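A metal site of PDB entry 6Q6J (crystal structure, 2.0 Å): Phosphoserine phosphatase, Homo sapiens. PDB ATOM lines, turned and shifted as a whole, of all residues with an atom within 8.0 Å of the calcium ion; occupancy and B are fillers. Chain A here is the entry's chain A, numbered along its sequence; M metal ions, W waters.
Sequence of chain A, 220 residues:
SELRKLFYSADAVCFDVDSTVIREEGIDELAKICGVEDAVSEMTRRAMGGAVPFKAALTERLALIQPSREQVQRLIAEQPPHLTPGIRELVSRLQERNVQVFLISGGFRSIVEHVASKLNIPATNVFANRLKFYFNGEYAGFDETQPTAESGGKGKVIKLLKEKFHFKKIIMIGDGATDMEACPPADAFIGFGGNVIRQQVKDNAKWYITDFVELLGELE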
ATOM      1  N   PHE A  15     -23.792 -15.533 -16.657  1.00  0.00           N
ATOM      2  CA  PHE A  15     -23.704 -15.964 -18.045  1.00  0.00           C
ATOM      3  C   PHE A  15     -22.261 -15.859 -18.513  1.00  0.00           C
ATOM      4  O   PHE A  15     -21.595 -14.851 -18.293  1.00  0.00           O
ATOM      5  CB  PHE A  15     -24.574 -15.105 -18.967  1.00  0.00           C
ATOM      6  CG  PHE A  15     -26.030 -15.390 -18.876  1.00  0.00           C
ATOM      7  CD1 PHE A  15     -26.616 -16.399 -19.630  1.00  0.00           C
ATOM      8  CD2 PHE A  15     -26.840 -14.632 -18.035  1.00  0.00           C
ATOM      9  CE1 PHE A  15     -27.952 -16.667 -19.541  1.00  0.00           C
ATOM     10  CE2 PHE A  15     -28.198 -14.874 -17.962  1.00  0.00           C
ATOM     11  CZ  PHE A  15     -28.766 -15.895 -18.699  1.00  0.00           C
ATOM     12  N   ASP A  16     -21.769 -16.912 -19.150  1.00  0.00           N
ATOM     13  CA  ASP A  16     -20.591 -16.785 -19.990  1.00  0.00           C
ATOM     14  C   ASP A  16     -20.917 -15.866 -21.150  1.00  0.00           C
ATOM     15  O   ASP A  16     -22.077 -15.730 -21.532  1.00  0.00           O
ATOM     16  CB  ASP A  16     -20.163 -18.180 -20.457  1.00  0.00           C
ATOM     17  CG  ASP A  16     -19.135 -18.157 -21.560  1.00  0.00           C
ATOM     18  OD1 ASP A  16     -18.113 -17.443 -21.456  1.00  0.00           O
ATOM     19  OD2 ASP A  16     -19.365 -18.884 -22.523  1.00  0.00           O
ATOM     20  N   VAL A  17     -19.912 -15.160 -21.690  1.00  0.00           N
ATOM     21  CA  VAL A  17     -20.233 -14.219 -22.767  1.00  0.00           C
ATOM     22  C   VAL A  17     -20.017 -14.843 -24.146  1.00  0.00           C
ATOM     23  O   VAL A  17     -20.980 -15.087 -24.885  1.00  0.00           O
ATOM     24  CB  VAL A  17     -19.460 -12.885 -22.613  1.00  0.00           C
ATOM     25  CG1 VAL A  17     -19.757 -11.972 -23.797  1.00  0.00           C
ATOM     26  CG2 VAL A  17     -19.862 -12.174 -21.318  1.00  0.00           C
ATOM     27  N   ASP A  18     -18.747 -15.141 -24.486  1.00  0.00           N
ATOM     28  CA  ASP A  18     -18.399 -15.673 -25.801  1.00  0.00           C
ATOM     29  C   ASP A  18     -19.133 -16.984 -26.099  1.00  0.00           C
ATOM     30  O   ASP A  18     -18.986 -17.974 -25.369  1.00  0.00           O
ATOM     31  CB  ASP A  18     -16.886 -15.906 -25.890  1.00  0.00           C
ATOM     32  CG  ASP A  18     -16.064 -14.592 -25.875  1.00  0.00           C
ATOM     33  OD1 ASP A  18     -16.584 -13.514 -26.222  1.00  0.00           O
ATOM     34  OD2 ASP A  18     -14.872 -14.652 -25.530  1.00  0.00           O
ATOM     35  N   SER A  19     -19.920 -17.006 -27.173  1.00  0.00           N
ATOM     36  CA  SER A  19     -20.672 -18.148 -27.666  1.00  0.00           C
ATOM     37  C   SER A  19     -21.886 -18.478 -26.819  1.00  0.00           C
ATOM     38  O   SER A  19     -22.601 -19.442 -27.141  1.00  0.00           O
ATOM     39  CB  SER A  19     -19.806 -19.415 -27.829  1.00  0.00           C
ATOM     40  OG  SER A  19     -18.756 -19.168 -28.745  1.00  0.00           O
ATOM     41  N   THR A  20     -22.169 -17.688 -25.773  1.00  0.00           N
ATOM     42  CA  THR A  20     -23.350 -17.872 -24.948  1.00  0.00           C
ATOM     43  C   THR A  20     -24.250 -16.640 -25.067  1.00  0.00           C
ATOM     44  O   THR A  20     -25.268 -16.705 -25.755  1.00  0.00           O
ATOM     45  CB  THR A  20     -22.969 -18.159 -23.490  1.00  0.00           C
ATOM     46  OG1 THR A  20     -22.209 -19.358 -23.402  1.00  0.00           O
ATOM     47  CG2 THR A  20     -24.203 -18.357 -22.639  1.00  0.00           C
ATOM     48  N   VAL A  21     -23.874 -15.514 -24.441  1.00  0.00           N
ATOM     49  CA  VAL A  21     -24.660 -14.286 -24.584  1.00  0.00           C
ATOM     50  C   VAL A  21     -24.543 -13.729 -26.006  1.00  0.00           C
ATOM     51  O   VAL A  21     -25.515 -13.177 -26.547  1.00  0.00           O
ATOM     52  CB  VAL A  21     -24.221 -13.266 -23.530  1.00  0.00           C
ATOM     53  CG1 VAL A  21     -24.831 -11.888 -23.792  1.00  0.00           C
ATOM     54  CG2 VAL A  21     -24.664 -13.774 -22.149  1.00  0.00           C
ATOM     55  N   ILE A  22     -23.384 -13.868 -26.633  1.00  0.00           N
ATOM     56  CA  ILE A  22     -23.188 -13.423 -28.012  1.00  0.00           C
ATOM     57  C   ILE A  22     -22.813 -14.611 -28.889  1.00  0.00           C
ATOM     58  O   ILE A  22     -22.340 -15.648 -28.403  1.00  0.00           O
ATOM     59  CB  ILE A  22     -22.109 -12.325 -28.134  1.00  0.00           C
ATOM     60  CG1 ILE A  22     -20.741 -12.851 -27.646  1.00  0.00           C
ATOM     61  CG2 ILE A  22     -22.516 -11.078 -27.390  1.00  0.00           C
ATOM     62  CD1 ILE A  22     -19.636 -11.794 -27.744  1.00  0.00           C
ATOM     63  N   GLU A  24     -20.439 -14.691 -31.083  1.00  0.00           N
ATOM     64  CA  GLU A  24     -19.036 -14.669 -31.462  1.00  0.00           C
ATOM     65  C   GLU A  24     -18.151 -14.868 -30.236  1.00  0.00           C
ATOM     66  O   GLU A  24     -18.616 -14.929 -29.088  1.00  0.00           O
ATOM     67  CB  GLU A  24     -18.699 -13.328 -32.137  1.00  0.00           C
ATOM     68  CG  GLU A  24     -19.540 -13.002 -33.388  1.00  0.00           C
ATOM     69  CD  GLU A  24     -20.666 -11.971 -33.125  1.00  0.00           C
ATOM     70  OE1 GLU A  24     -21.168 -11.887 -31.971  1.00  0.00           O
ATOM     71  OE2 GLU A  24     -21.052 -11.252 -34.072  1.00  0.00           O
ATOM     72  N   GLU A  25     -16.851 -14.994 -30.504  1.00  0.00           N
ATOM     73  CA  GLU A  25     -15.801 -14.906 -29.495  1.00  0.00           C
ATOM     74  C   GLU A  25     -15.195 -13.519 -29.611  1.00  0.00           C
ATOM     75  O   GLU A  25     -14.686 -13.152 -30.688  1.00  0.00           O
ATOM     76  CB  GLU A  25     -14.756 -16.003 -29.694  1.00  0.00           C
ATOM     77  CG  GLU A  25     -13.935 -16.376 -28.454  1.00  0.00           C
ATOM     78  CD  GLU A  25     -14.469 -17.612 -27.708  1.00  0.00           C
ATOM     79  OE1 GLU A  25     -13.962 -17.919 -26.579  1.00  0.00           O
ATOM     80  OE2 GLU A  25     -15.408 -18.257 -28.241  1.00  0.00           O
ATOM     81  N   MET A  48      -9.781 -23.822 -25.661  1.00  0.00           N
ATOM     82  CA  MET A  48     -11.118 -24.152 -25.194  1.00  0.00           C
ATOM     83  C   MET A  48     -11.091 -25.424 -24.352  1.00  0.00           C
ATOM     84  O   MET A  48     -10.375 -26.387 -24.664  1.00  0.00           O
ATOM     85  CB  MET A  48     -12.095 -24.325 -26.370  1.00  0.00           C
ATOM     86  CG  MET A  48     -12.586 -23.023 -26.994  1.00  0.00           C
ATOM     87  SD  MET A  48     -13.399 -21.847 -25.866  1.00  0.00           S
ATOM     88  CE  MET A  48     -14.746 -22.831 -25.189  1.00  0.00           C
ATOM     89  N   ILE A 104     -19.649 -12.875 -17.068  1.00  0.00           N
ATOM     90  CA  ILE A 104     -18.289 -13.250 -16.718  1.00  0.00           C
ATOM     91  C   ILE A 104     -17.632 -13.747 -17.984  1.00  0.00           C
ATOM     92  O   ILE A 104     -18.185 -14.610 -18.679  1.00  0.00           O
ATOM     93  CB  ILE A 104     -18.248 -14.328 -15.620  1.00  0.00           C
ATOM     94  CG1 ILE A 104     -19.196 -13.986 -14.464  1.00  0.00           C
ATOM     95  CG2 ILE A 104     -16.793 -14.540 -15.125  1.00  0.00           C
ATOM     96  CD1 ILE A 104     -19.196 -15.061 -13.402  1.00  0.00           C
ATOM     97  N   SER A 105     -16.457 -13.190 -18.293  1.00  0.00           N
ATOM     98  CA  SER A 105     -15.821 -13.518 -19.563  1.00  0.00           C
ATOM     99  C   SER A 105     -14.313 -13.473 -19.407  1.00  0.00           C
ATOM    100  O   SER A 105     -13.785 -12.665 -18.643  1.00  0.00           O
ATOM    101  CB  SER A 105     -16.270 -12.529 -20.653  1.00  0.00           C
ATOM    102  OG  SER A 105     -15.599 -12.795 -21.882  1.00  0.00           O
ATOM    103  N   GLY A 106     -13.627 -14.353 -20.143  1.00  0.00           N
ATOM    104  CA  GLY A 106     -12.213 -14.160 -20.338  1.00  0.00           C
ATOM    105  C   GLY A 106     -11.889 -13.143 -21.401  1.00  0.00           C
ATOM    106  O   GLY A 106     -10.718 -12.861 -21.662  1.00  0.00           O
ATOM    107  N   LYS A 154     -13.485 -18.034 -13.607  1.00  0.00           N
ATOM    108  CA  LYS A 154     -14.929 -17.955 -13.437  1.00  0.00           C
ATOM    109  C   LYS A 154     -15.367 -18.468 -12.076  1.00  0.00           C
ATOM    110  O   LYS A 154     -16.254 -17.886 -11.433  1.00  0.00           O
ATOM    111  CB  LYS A 154     -15.640 -18.712 -14.550  1.00  0.00           C
ATOM    112  CG  LYS A 154     -15.561 -18.010 -15.904  1.00  0.00           C
ATOM    113  CD  LYS A 154     -16.142 -18.841 -17.038  1.00  0.00           C
ATOM    114  CE  LYS A 154     -16.107 -18.050 -18.360  1.00  0.00           C
ATOM    115  NZ  LYS A 154     -16.326 -18.939 -19.550  1.00  0.00           N
ATOM    116  N   MET A 172     -24.582 -20.961 -13.057  1.00  0.00           N
ATOM    117  CA  MET A 172     -23.668 -20.622 -14.132  1.00  0.00           C
ATOM    118  C   MET A 172     -24.258 -21.169 -15.423  1.00  0.00           C
ATOM    119  O   MET A 172     -24.693 -22.332 -15.460  1.00  0.00           O
ATOM    120  CB  MET A 172     -22.272 -21.212 -13.874  1.00  0.00           C
ATOM    121  CG  MET A 172     -21.301 -20.970 -15.025  1.00  0.00           C
ATOM    122  SD  MET A 172     -20.676 -19.298 -14.927  1.00  0.00           S
ATOM    123  CE  MET A 172     -20.425 -18.899 -16.659  1.00  0.00           C
ATOM    124  N   ILE A 173     -24.314 -20.333 -16.459  1.00  0.00           N
ATOM    125  CA  ILE A 173     -24.811 -20.713 -17.777  1.00  0.00           C
ATOM    126  C   ILE A 173     -23.712 -20.426 -18.776  1.00  0.00           C
ATOM    127  O   ILE A 173     -23.178 -19.315 -18.816  1.00  0.00           O
ATOM    128  CB  ILE A 173     -26.094 -19.958 -18.155  1.00  0.00           C
ATOM    129  CG1 ILE A 173     -27.183 -20.168 -17.110  1.00  0.00           C
ATOM    130  CG2 ILE A 173     -26.586 -20.400 -19.570  1.00  0.00           C
ATOM    131  CD1 ILE A 173     -28.547 -19.623 -17.507  1.00  0.00           C
ATOM    132  N   GLY A 174     -23.360 -21.432 -19.575  1.00  0.00           N
ATOM    133  CA  GLY A 174     -22.268 -21.260 -20.523  1.00  0.00           C
ATOM    134  C   GLY A 174     -22.102 -22.466 -21.419  1.00  0.00           C
ATOM    135  O   GLY A 174     -22.703 -23.520 -21.216  1.00  0.00           O
ATOM    136  N   ASP A 175     -21.267 -22.279 -22.447  1.00  0.00           N
ATOM    137  CA  ASP A 175     -21.159 -23.277 -23.501  1.00  0.00           C
ATOM    138  C   ASP A 175     -19.977 -24.240 -23.340  1.00  0.00           C
ATOM    139  O   ASP A 175     -19.992 -25.317 -23.953  1.00  0.00           O
ATOM    140  CB  ASP A 175     -21.007 -22.576 -24.854  1.00  0.00           C
ATOM    141  CG  ASP A 175     -19.689 -21.889 -24.966  1.00  0.00           C
ATOM    142  OD1 ASP A 175     -18.863 -22.273 -25.818  1.00  0.00           O
ATOM    143  OD2 ASP A 175     -19.451 -20.986 -24.141  1.00  0.00           O
ATOM    144  N   GLY A 176     -18.964 -23.898 -22.538  1.00  0.00           N
ATOM    145  CA  GLY A 176     -17.699 -24.603 -22.537  1.00  0.00           C
ATOM    146  C   GLY A 176     -17.345 -25.279 -21.230  1.00  0.00           C
ATOM    147  O   GLY A 176     -18.018 -25.129 -20.202  1.00  0.00           O
ATOM    148  N   ALA A 177     -16.234 -26.037 -21.287  1.00  0.00           N
ATOM    149  CA  ALA A 177     -15.781 -26.802 -20.119  1.00  0.00           C
ATOM    150  C   ALA A 177     -15.471 -25.900 -18.938  1.00  0.00           C
ATOM    151  O   ALA A 177     -15.775 -26.248 -17.792  1.00  0.00           O
ATOM    152  CB  ALA A 177     -14.555 -27.658 -20.479  1.00  0.00           C
ATOM    153  N   THR A 178     -14.870 -24.726 -19.182  1.00  0.00           N
ATOM    154  CA  THR A 178     -14.551 -23.806 -18.092  1.00  0.00           C
ATOM    155  C   THR A 178     -15.801 -23.272 -17.402  1.00  0.00           C
ATOM    156  O   THR A 178     -15.762 -22.947 -16.208  1.00  0.00           O
ATOM    157  CB  THR A 178     -13.688 -22.647 -18.589  1.00  0.00           C
ATOM    158  OG1 THR A 178     -14.498 -21.686 -19.266  1.00  0.00           O
ATOM    159  CG2 THR A 178     -12.590 -23.150 -19.512  1.00  0.00           C
ATOM    160  N   ASP A 179     -16.929 -23.168 -18.114  1.00  0.00           N
ATOM    161  CA  ASP A 179     -18.176 -22.804 -17.458  1.00  0.00           C
ATOM    162  C   ASP A 179     -18.672 -23.957 -16.598  1.00  0.00           C
ATOM    163  O   ASP A 179     -19.073 -23.760 -15.436  1.00  0.00           O
ATOM    164  CB  ASP A 179     -19.213 -22.409 -18.489  1.00  0.00           C
ATOM    165  CG  ASP A 179     -18.683 -21.410 -19.477  1.00  0.00           C
ATOM    166  OD1 ASP A 179     -18.355 -20.287 -19.058  1.00  0.00           O
ATOM    167  OD2 ASP A 179     -18.548 -21.765 -20.662  1.00  0.00           O
ATOM    168  N   PHE A 192     -25.027 -24.515 -22.570  1.00  0.00           N
ATOM    169  CA  PHE A 192     -25.718 -23.822 -23.646  1.00  0.00           C
ATOM    170  C   PHE A 192     -25.104 -24.181 -24.997  1.00  0.00           C
ATOM    171  O   PHE A 192     -23.924 -23.929 -25.231  1.00  0.00           O
ATOM    172  CB  PHE A 192     -25.677 -22.303 -23.465  1.00  0.00           C
ATOM    173  CG  PHE A 192     -26.457 -21.563 -24.537  1.00  0.00           C
ATOM    174  CD1 PHE A 192     -27.849 -21.649 -24.568  1.00  0.00           C
ATOM    175  CD2 PHE A 192     -25.802 -20.838 -25.511  1.00  0.00           C
ATOM    176  CE1 PHE A 192     -28.574 -21.006 -25.575  1.00  0.00           C
ATOM    177  CE2 PHE A 192     -26.507 -20.184 -26.518  1.00  0.00           C
ATOM    178  CZ  PHE A 192     -27.908 -20.264 -26.548  1.00  0.00           C
ATOM    179  N   VAL A 196     -22.878 -23.214 -30.541  1.00  0.00           N
ATOM    180  CA  VAL A 196     -22.058 -24.340 -30.959  1.00  0.00           C
ATOM    181  C   VAL A 196     -22.162 -25.395 -29.873  1.00  0.00           C
ATOM    182  O   VAL A 196     -22.069 -25.082 -28.676  1.00  0.00           O
ATOM    183  CB  VAL A 196     -20.592 -23.942 -31.213  1.00  0.00           C
ATOM    184  CG1 VAL A 196     -19.995 -23.243 -29.971  1.00  0.00           C
ATOM    185  CG2 VAL A 196     -19.752 -25.166 -31.631  1.00  0.00           C
ATOM    186  N   ARG A 198     -20.703 -28.067 -27.754  1.00  0.00           N
ATOM    187  CA  ARG A 198     -19.496 -28.726 -27.269  1.00  0.00           C
ATOM    188  C   ARG A 198     -19.962 -30.029 -26.647  1.00  0.00           C
ATOM    189  O   ARG A 198     -20.490 -30.048 -25.539  1.00  0.00           O
ATOM    190  CB  ARG A 198     -18.733 -27.835 -26.302  1.00  0.00           C
ATOM    191  CG  ARG A 198     -18.247 -26.593 -26.992  1.00  0.00           C
ATOM    192  CD  ARG A 198     -17.296 -25.741 -26.191  1.00  0.00           C
ATOM    193  NE  ARG A 198     -17.298 -24.369 -26.703  1.00  0.00           N
ATOM    194  CZ  ARG A 198     -16.556 -23.941 -27.711  1.00  0.00           C
ATOM    195  NH1 ARG A 198     -15.715 -24.768 -28.319  1.00  0.00           N
ATOM    196  NH2 ARG A 198     -16.632 -22.677 -28.093  1.00  0.00           N
HETATM  197 CA    CA M   1     -17.851 -19.419 -24.021  1.00  0.00          CA
HETATM  198  O   HOH W   1     -15.813 -18.384 -23.732  1.00  0.00           O
HETATM  199  O   HOH W   2     -16.699 -19.999 -25.977  1.00  0.00           O
HETATM  200  O   HOH W   3     -16.906 -20.861 -22.298  1.00  0.00           O
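OG1 of Thr 20 lies close to OD2 of Asp 16, 3.0 Å away. NZ of Lys 154 lies within salt-bridge range of OD1 of Asp 16 (3.0 Å). The backbone NH (N) of Val 21 sits close to the backbone carbonyl oxygen (O) of Asp 16. The backbone carbonyl oxygen (O) of Ile 173 lies within hydrogen-bond range of the backbone NH (N) of Asp 16. OD2 of Asp 179 lies within hydrogen-bond range of N of Asp 175 (3.3 Å). The backbone NH of Asp 175 sits at hydrogen-bond distance from the side-chain hydroxyl of Thr 20. The side-chain carboxylate (OD1) of Asp 175 is in salt-bridge range of the guanidinium group (NE) of Arg 198 (2.8 Å).
Three residues have an atom within 4 Å of the calcium ion: Asp 16, Asp 18 and Asp 175.
The side-chain carboxylate (OD2) of Asp 16 binds the calcium ion (2.2 Å). The calcium ion is bound by the side-chain carboxylate (OD2) of Asp 175. The calcium ion is bound by O of Asp 18 (2.3 Å). Water W1 binds the calcium ion, 2.3 Å away. The calcium ion is bound by water W2, at 2.3 Å. Water W3 binds the calcium ion, 2.4 Å away. The calcium ion has six donor atoms within binding distance.
Water W3 bridges OD2 of Asp 179 and NZ of Lys 154. Water W1 lies within hydrogen-bond range of OD1 of Asp 16 (3.4 Å) and OE1 of Glu 25 (3.4 Å).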
